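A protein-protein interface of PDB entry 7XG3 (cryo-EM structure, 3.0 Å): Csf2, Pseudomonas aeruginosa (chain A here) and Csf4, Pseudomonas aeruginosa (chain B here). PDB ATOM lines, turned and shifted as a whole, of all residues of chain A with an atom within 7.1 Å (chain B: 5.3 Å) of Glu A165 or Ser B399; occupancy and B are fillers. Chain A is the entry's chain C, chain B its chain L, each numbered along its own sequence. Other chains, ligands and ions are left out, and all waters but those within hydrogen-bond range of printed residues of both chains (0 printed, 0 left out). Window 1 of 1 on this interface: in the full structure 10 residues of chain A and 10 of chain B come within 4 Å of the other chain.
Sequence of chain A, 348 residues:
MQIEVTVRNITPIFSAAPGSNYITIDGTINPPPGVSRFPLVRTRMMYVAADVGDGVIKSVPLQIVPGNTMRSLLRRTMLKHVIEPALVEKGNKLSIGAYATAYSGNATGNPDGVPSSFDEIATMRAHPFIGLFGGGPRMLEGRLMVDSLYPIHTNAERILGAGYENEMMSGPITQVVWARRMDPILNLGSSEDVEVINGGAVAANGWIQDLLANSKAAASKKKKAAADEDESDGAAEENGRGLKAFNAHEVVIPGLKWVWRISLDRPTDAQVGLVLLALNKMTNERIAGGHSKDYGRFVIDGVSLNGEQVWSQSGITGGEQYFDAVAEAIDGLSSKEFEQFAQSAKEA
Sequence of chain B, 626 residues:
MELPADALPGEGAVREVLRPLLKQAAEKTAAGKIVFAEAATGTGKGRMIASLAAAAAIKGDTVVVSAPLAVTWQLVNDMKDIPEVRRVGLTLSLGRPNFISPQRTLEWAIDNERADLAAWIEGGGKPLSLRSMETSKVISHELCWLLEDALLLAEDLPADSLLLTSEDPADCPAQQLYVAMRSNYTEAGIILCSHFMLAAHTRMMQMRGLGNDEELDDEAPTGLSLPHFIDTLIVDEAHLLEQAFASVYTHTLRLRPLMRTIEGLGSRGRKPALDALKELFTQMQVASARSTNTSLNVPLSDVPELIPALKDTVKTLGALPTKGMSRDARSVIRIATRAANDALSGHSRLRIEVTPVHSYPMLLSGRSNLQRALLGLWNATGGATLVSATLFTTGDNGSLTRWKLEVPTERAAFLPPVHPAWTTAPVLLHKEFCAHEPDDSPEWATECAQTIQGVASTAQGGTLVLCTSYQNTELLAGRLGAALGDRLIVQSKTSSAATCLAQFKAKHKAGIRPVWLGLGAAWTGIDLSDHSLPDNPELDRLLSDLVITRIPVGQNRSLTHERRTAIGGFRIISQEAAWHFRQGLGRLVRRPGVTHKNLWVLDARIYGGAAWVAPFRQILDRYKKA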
ATOM      1  N   ILE A 152      -4.772  27.956  16.176  1.00  0.00           N
ATOM      2  CA  ILE A 152      -5.878  27.806  15.241  1.00  0.00           C
ATOM      3  C   ILE A 152      -7.044  27.181  15.995  1.00  0.00           C
ATOM      4  O   ILE A 152      -7.135  25.956  16.131  1.00  0.00           O
ATOM      5  CB  ILE A 152      -5.464  26.973  14.021  1.00  0.00           C
ATOM      6  CG1 ILE A 152      -4.109  27.461  13.501  1.00  0.00           C
ATOM      7  CG2 ILE A 152      -6.530  27.068  12.937  1.00  0.00           C
ATOM      8  CD1 ILE A 152      -3.693  26.890  12.161  1.00  0.00           C
ATOM      9  N   THR A 154     -11.386  27.746  17.435  1.00  0.00           N
ATOM     10  CA  THR A 154     -12.686  28.300  17.069  1.00  0.00           C
ATOM     11  C   THR A 154     -13.033  29.530  17.900  1.00  0.00           C
ATOM     12  O   THR A 154     -13.898  30.323  17.511  1.00  0.00           O
ATOM     13  CB  THR A 154     -13.776  27.239  17.217  1.00  0.00           C
ATOM     14  OG1 THR A 154     -15.049  27.816  16.901  1.00  0.00           O
ATOM     15  CG2 THR A 154     -13.810  26.698  18.633  1.00  0.00           C
ATOM     16  N   GLU A 157     -11.653  32.606  15.797  1.00  0.00           N
ATOM     17  CA  GLU A 157     -12.033  32.694  14.386  1.00  0.00           C
ATOM     18  C   GLU A 157     -12.197  34.140  13.927  1.00  0.00           C
ATOM     19  O   GLU A 157     -12.051  34.441  12.737  1.00  0.00           O
ATOM     20  CB  GLU A 157     -13.316  31.906  14.131  1.00  0.00           C
ATOM     21  CG  GLU A 157     -13.088  30.421  13.923  1.00  0.00           C
ATOM     22  CD  GLU A 157     -14.356  29.688  13.544  1.00  0.00           C
ATOM     23  OE1 GLU A 157     -15.446  30.279  13.672  1.00  0.00           O
ATOM     24  OE2 GLU A 157     -14.261  28.523  13.107  1.00  0.00           O
ATOM     25  N   GLY A 161      -9.440  34.712  11.209  1.00  0.00           N
ATOM     26  CA  GLY A 161     -10.044  35.074   9.913  1.00  0.00           C
ATOM     27  C   GLY A 161     -10.436  33.832   9.127  1.00  0.00           C
ATOM     28  O   GLY A 161     -10.256  32.714   9.650  1.00  0.00           O
ATOM     29  N   ALA A 162     -10.975  34.015   7.919  1.00  0.00           N
ATOM     30  CA  ALA A 162     -11.389  32.873   7.071  1.00  0.00           C
ATOM     31  C   ALA A 162     -10.161  32.178   6.469  1.00  0.00           C
ATOM     32  O   ALA A 162      -9.096  32.820   6.384  1.00  0.00           O
ATOM     33  CB  ALA A 162     -12.349  33.337   6.002  1.00  0.00           C
ATOM     34  N   GLY A 163     -10.304  30.899   6.107  1.00  0.00           N
ATOM     35  CA  GLY A 163      -9.233  30.149   5.500  1.00  0.00           C
ATOM     36  C   GLY A 163      -8.550  29.152   6.410  1.00  0.00           C
ATOM     37  O   GLY A 163      -7.896  28.230   5.913  1.00  0.00           O
ATOM     38  N   TYR A 164      -8.686  29.308   7.723  1.00  0.00           N
ATOM     39  CA  TYR A 164      -8.125  28.369   8.682  1.00  0.00           C
ATOM     40  C   TYR A 164      -9.154  27.385   9.201  1.00  0.00           C
ATOM     41  O   TYR A 164      -8.883  26.686  10.184  1.00  0.00           O
ATOM     42  CB  TYR A 164      -7.493  29.131   9.848  1.00  0.00           C
ATOM     43  CG  TYR A 164      -6.354  30.008   9.412  1.00  0.00           C
ATOM     44  CD1 TYR A 164      -5.094  29.476   9.168  1.00  0.00           C
ATOM     45  CD2 TYR A 164      -6.533  31.372   9.255  1.00  0.00           C
ATOM     46  CE1 TYR A 164      -4.053  30.284   8.773  1.00  0.00           C
ATOM     47  CE2 TYR A 164      -5.506  32.185   8.866  1.00  0.00           C
ATOM     48  CZ  TYR A 164      -4.271  31.637   8.626  1.00  0.00           C
ATOM     49  OH  TYR A 164      -3.252  32.457   8.233  1.00  0.00           O
ATOM     50  N   GLU A 165     -10.331  27.328   8.570  1.00  0.00           N
ATOM     51  CA  GLU A 165     -11.381  26.406   8.984  1.00  0.00           C
ATOM     52  C   GLU A 165     -10.955  24.959   8.773  1.00  0.00           C
ATOM     53  O   GLU A 165     -11.268  24.082   9.582  1.00  0.00           O
ATOM     54  CB  GLU A 165     -12.666  26.716   8.218  1.00  0.00           C
ATOM     55  CG  GLU A 165     -12.981  28.200   8.104  1.00  0.00           C
ATOM     56  CD  GLU A 165     -13.704  28.747   9.319  1.00  0.00           C
ATOM     57  OE1 GLU A 165     -14.141  27.945  10.170  1.00  0.00           O
ATOM     58  OE2 GLU A 165     -13.837  29.985   9.420  1.00  0.00           O
ATOM     59  N   ASN A 166     -10.250  24.688   7.679  1.00  0.00           N
ATOM     60  CA  ASN A 166      -9.544  23.421   7.558  1.00  0.00           C
ATOM     61  C   ASN A 166      -8.354  23.428   8.506  1.00  0.00           C
ATOM     62  O   ASN A 166      -7.697  24.461   8.679  1.00  0.00           O
ATOM     63  CB  ASN A 166      -9.085  23.194   6.117  1.00  0.00           C
ATOM     64  CG  ASN A 166      -8.629  21.765   5.861  1.00  0.00           C
ATOM     65  OD1 ASN A 166      -8.772  20.890   6.716  1.00  0.00           O
ATOM     66  ND2 ASN A 166      -8.085  21.522   4.675  1.00  0.00           N
ATOM     67  N   GLU A 167      -8.098  22.272   9.132  1.00  0.00           N
ATOM     68  CA  GLU A 167      -7.031  22.058  10.119  1.00  0.00           C
ATOM     69  C   GLU A 167      -7.179  23.028  11.298  1.00  0.00           C
ATOM     70  O   GLU A 167      -6.374  23.932  11.527  1.00  0.00           O
ATOM     71  CB  GLU A 167      -5.647  22.143   9.462  1.00  0.00           C
ATOM     72  CG  GLU A 167      -4.595  21.277  10.114  1.00  0.00           C
ATOM     73  CD  GLU A 167      -3.883  22.002  11.222  1.00  0.00           C
ATOM     74  OE1 GLU A 167      -3.591  23.200  11.031  1.00  0.00           O
ATOM     75  OE2 GLU A 167      -3.618  21.384  12.274  1.00  0.00           O
ATOM     76  N   MET A 168      -8.266  22.808  12.033  1.00  0.00           N
ATOM     77  CA  MET A 168      -8.755  23.719  13.055  1.00  0.00           C
ATOM     78  C   MET A 168      -9.080  22.912  14.307  1.00  0.00           C
ATOM     79  O   MET A 168      -9.585  21.790  14.228  1.00  0.00           O
ATOM     80  CB  MET A 168      -9.987  24.467  12.526  1.00  0.00           C
ATOM     81  CG  MET A 168     -10.890  25.121  13.545  1.00  0.00           C
ATOM     82  SD  MET A 168     -10.175  26.623  14.185  1.00  0.00           S
ATOM     83  CE  MET A 168     -10.494  27.774  12.863  1.00  0.00           C
ATOM     84  N   MET A 169      -8.765  23.475  15.473  1.00  0.00           N
ATOM     85  CA  MET A 169      -9.117  22.856  16.742  1.00  0.00           C
ATOM     86  C   MET A 169     -10.310  23.548  17.384  1.00  0.00           C
ATOM     87  O   MET A 169     -10.719  24.644  16.994  1.00  0.00           O
ATOM     88  CB  MET A 169      -7.946  22.837  17.730  1.00  0.00           C
ATOM     89  CG  MET A 169      -6.947  21.735  17.474  1.00  0.00           C
ATOM     90  SD  MET A 169      -6.321  21.147  19.059  1.00  0.00           S
ATOM     91  CE  MET A 169      -7.786  20.394  19.742  1.00  0.00           C
ATOM     92  N   THR B 393     -23.299  32.420   4.201  1.00  0.00           N
ATOM     93  CA  THR B 393     -23.787  31.956   5.492  1.00  0.00           C
ATOM     94  C   THR B 393     -24.608  33.030   6.201  1.00  0.00           C
ATOM     95  O   THR B 393     -25.812  32.860   6.430  1.00  0.00           O
ATOM     96  CB  THR B 393     -22.597  31.500   6.340  1.00  0.00           C
ATOM     97  OG1 THR B 393     -22.042  30.305   5.777  1.00  0.00           O
ATOM     98  CG2 THR B 393     -23.036  31.178   7.723  1.00  0.00           C
ATOM     99  N   ASN B 397     -20.404  36.580   5.225  1.00  0.00           N
ATOM    100  CA  ASN B 397     -19.601  35.418   5.601  1.00  0.00           C
ATOM    101  C   ASN B 397     -19.877  34.261   4.649  1.00  0.00           C
ATOM    102  O   ASN B 397     -21.016  33.796   4.547  1.00  0.00           O
ATOM    103  CB  ASN B 397     -19.884  34.974   7.032  1.00  0.00           C
ATOM    104  CG  ASN B 397     -18.995  33.816   7.465  1.00  0.00           C
ATOM    105  OD1 ASN B 397     -19.405  32.658   7.390  1.00  0.00           O
ATOM    106  ND2 ASN B 397     -17.782  34.117   7.917  1.00  0.00           N
ATOM    107  N   GLY B 398     -18.841  33.801   3.955  1.00  0.00           N
ATOM    108  CA  GLY B 398     -18.915  32.570   3.194  1.00  0.00           C
ATOM    109  C   GLY B 398     -17.734  31.660   3.475  1.00  0.00           C
ATOM    110  O   GLY B 398     -17.198  31.026   2.562  1.00  0.00           O
ATOM    111  N   SER B 399     -17.315  31.608   4.744  1.00  0.00           N
ATOM    112  CA  SER B 399     -16.094  30.890   5.109  1.00  0.00           C
ATOM    113  C   SER B 399     -16.265  29.381   4.984  1.00  0.00           C
ATOM    114  O   SER B 399     -15.346  28.675   4.539  1.00  0.00           O
ATOM    115  CB  SER B 399     -15.681  31.259   6.532  1.00  0.00           C
ATOM    116  OG  SER B 399     -16.814  31.334   7.378  1.00  0.00           O
ATOM    117  N   LEU B 400     -17.433  28.862   5.369  1.00  0.00           N
ATOM    118  CA  LEU B 400     -17.663  27.430   5.218  1.00  0.00           C
ATOM    119  C   LEU B 400     -17.791  27.062   3.751  1.00  0.00           C
ATOM    120  O   LEU B 400     -17.537  25.918   3.379  1.00  0.00           O
ATOM    121  CB  LEU B 400     -18.904  26.990   5.999  1.00  0.00           C
ATOM    122  CG  LEU B 400     -20.361  27.052   5.504  1.00  0.00           C
ATOM    123  CD1 LEU B 400     -20.839  25.860   4.656  1.00  0.00           C
ATOM    124  CD2 LEU B 400     -21.244  27.199   6.675  1.00  0.00           C
ATOM    125  N   THR B 401     -18.207  28.014   2.912  1.00  0.00           N
ATOM    126  CA  THR B 401     -18.347  27.730   1.491  1.00  0.00           C
ATOM    127  C   THR B 401     -16.996  27.464   0.854  1.00  0.00           C
ATOM    128  O   THR B 401     -16.823  26.474   0.137  1.00  0.00           O
ATOM    129  CB  THR B 401     -19.007  28.889   0.770  1.00  0.00           C
ATOM    130  OG1 THR B 401     -20.015  29.462   1.601  1.00  0.00           O
ATOM    131  CG2 THR B 401     -19.658  28.348  -0.457  1.00  0.00           C
ATOM    132  N   ARG B 402     -16.014  28.319   1.136  1.00  0.00           N
ATOM    133  CA  ARG B 402     -14.660  28.045   0.684  1.00  0.00           C
ATOM    134  C   ARG B 402     -14.005  26.929   1.493  1.00  0.00           C
ATOM    135  O   ARG B 402     -12.918  26.471   1.135  1.00  0.00           O
ATOM    136  CB  ARG B 402     -13.820  29.323   0.721  1.00  0.00           C
ATOM    137  CG  ARG B 402     -13.712  29.973   2.075  1.00  0.00           C
ATOM    138  CD  ARG B 402     -12.299  30.476   2.333  1.00  0.00           C
ATOM    139  NE  ARG B 402     -11.282  29.484   1.990  1.00  0.00           N
ATOM    140  CZ  ARG B 402     -10.995  28.405   2.709  1.00  0.00           C
ATOM    141  NH1 ARG B 402     -11.625  28.133   3.843  1.00  0.00           N
ATOM    142  NH2 ARG B 402     -10.045  27.578   2.285  1.00  0.00           N
ATOM    143  N   TRP B 403     -14.630  26.493   2.594  1.00  0.00           N
ATOM    144  CA  TRP B 403     -14.211  25.235   3.209  1.00  0.00           C
ATOM    145  C   TRP B 403     -14.721  24.000   2.449  1.00  0.00           C
ATOM    146  O   TRP B 403     -13.971  23.028   2.312  1.00  0.00           O
ATOM    147  CB  TRP B 403     -14.650  25.212   4.678  1.00  0.00           C
ATOM    148  CG  TRP B 403     -14.061  24.115   5.530  1.00  0.00           C
ATOM    149  CD1 TRP B 403     -13.023  23.287   5.214  1.00  0.00           C
ATOM    150  CD2 TRP B 403     -14.447  23.777   6.867  1.00  0.00           C
ATOM    151  NE1 TRP B 403     -12.767  22.429   6.254  1.00  0.00           N
ATOM    152  CE2 TRP B 403     -13.623  22.715   7.283  1.00  0.00           C
ATOM    153  CE3 TRP B 403     -15.422  24.262   7.747  1.00  0.00           C
ATOM    154  CZ2 TRP B 403     -13.745  22.127   8.537  1.00  0.00           C
ATOM    155  CZ3 TRP B 403     -15.534  23.682   8.996  1.00  0.00           C
ATOM    156  CH2 TRP B 403     -14.699  22.627   9.380  1.00  0.00           C
ATOM    157  N   PHE B 414     -15.130  37.751  -1.973  1.00  0.00           N
ATOM    158  CA  PHE B 414     -16.438  37.683  -1.319  1.00  0.00           C
ATOM    159  C   PHE B 414     -17.212  38.942  -1.688  1.00  0.00           C
ATOM    160  O   PHE B 414     -16.956  40.019  -1.142  1.00  0.00           O
ATOM    161  CB  PHE B 414     -16.307  37.553   0.202  1.00  0.00           C
ATOM    162  CG  PHE B 414     -15.924  36.166   0.704  1.00  0.00           C
ATOM    163  CD1 PHE B 414     -15.137  35.294  -0.039  1.00  0.00           C
ATOM    164  CD2 PHE B 414     -16.364  35.748   1.952  1.00  0.00           C
ATOM    165  CE1 PHE B 414     -14.801  34.044   0.448  1.00  0.00           C
ATOM    166  CE2 PHE B 414     -16.020  34.503   2.449  1.00  0.00           C
ATOM    167  CZ  PHE B 414     -15.246  33.649   1.690  1.00  0.00           C
ATOM    168  N   ILE B 567     -14.770  18.568  12.513  1.00  0.00           N
ATOM    169  CA  ILE B 567     -13.852  19.673  12.769  1.00  0.00           C
ATOM    170  C   ILE B 567     -14.595  20.860  13.369  1.00  0.00           C
ATOM    171  O   ILE B 567     -14.233  21.361  14.439  1.00  0.00           O
ATOM    172  CB  ILE B 567     -13.115  20.083  11.479  1.00  0.00           C
ATOM    173  CG1 ILE B 567     -12.449  18.878  10.821  1.00  0.00           C
ATOM    174  CG2 ILE B 567     -12.103  21.175  11.780  1.00  0.00           C
ATOM    175  CD1 ILE B 567     -11.747  19.195   9.522  1.00  0.00           C
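Of chain B, only Ser B399, Trp B403 and Ile B567 come within 4 Å of Glu A165.
Ser B399 touches two residues of chain A.
No residue of chain A comes within 4 Å of Gly B398.
Of the printed residues of chain A, Arg B402 touches Gly A163 (3.5 Å).
Of the printed residues of chain B, Ala A162 touches Ser B399.
Of the printed residues of chain B, Gly A163 touches Arg B402 (3.5 Å).
Printed residues of chain B within 4 Å of Asn A166: Trp B403.
Of the printed residues of chain A, Trp B403 touches Glu A165 (3.3 Å) and Asn A166 (3.6 Å).
The nearest printed residue of chain B that does not touch Ala A162 is Arg B402 (4.7 Å).
Ser B399 touches Ala A162.
Arg B402 touches Gly A163.
Glu A165 touches Ser B399 (OE2 to CB, 3.7 Å).
Trp B403 touches Glu A165 (CZ2 to O, 3.3 Å).
Glu A165 touches Ile B567 (O to CG2, 3.7 Å).
Asn A166 touches Trp B403 (CA to NE1, 3.6 Å).
Met A168 touches Ile B567 (O to CG2, 3.6 Å).
Printed residues of chain A that touch a printed residue of chain B: Ala A162, Gly A163, Glu A165, Asn A166 and Met A168.
Of the 10 printed residues of chain B, 4 touch a printed residue of chain A.
Printed residues of chain B that touch a printed residue of chain A: Ser B399, Arg B402, Trp B403 and Ile B567.
Hydrophobic or aromatic side chains of chain B within 4 Å of the printed part of chain A: Trp B403 and Ile B567.
Along chain B the printed residues that touch a printed residue of chain A span positions 399 to 567.
The side-chain sulfur (SD) of Met A168 sits at hydrogen-bond distance from the backbone NH (N) of Thr A154 (3.6 Å).
OD1 of Asn B397 sits at hydrogen-bond distance from OG of Ser B399 (2.9 Å).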
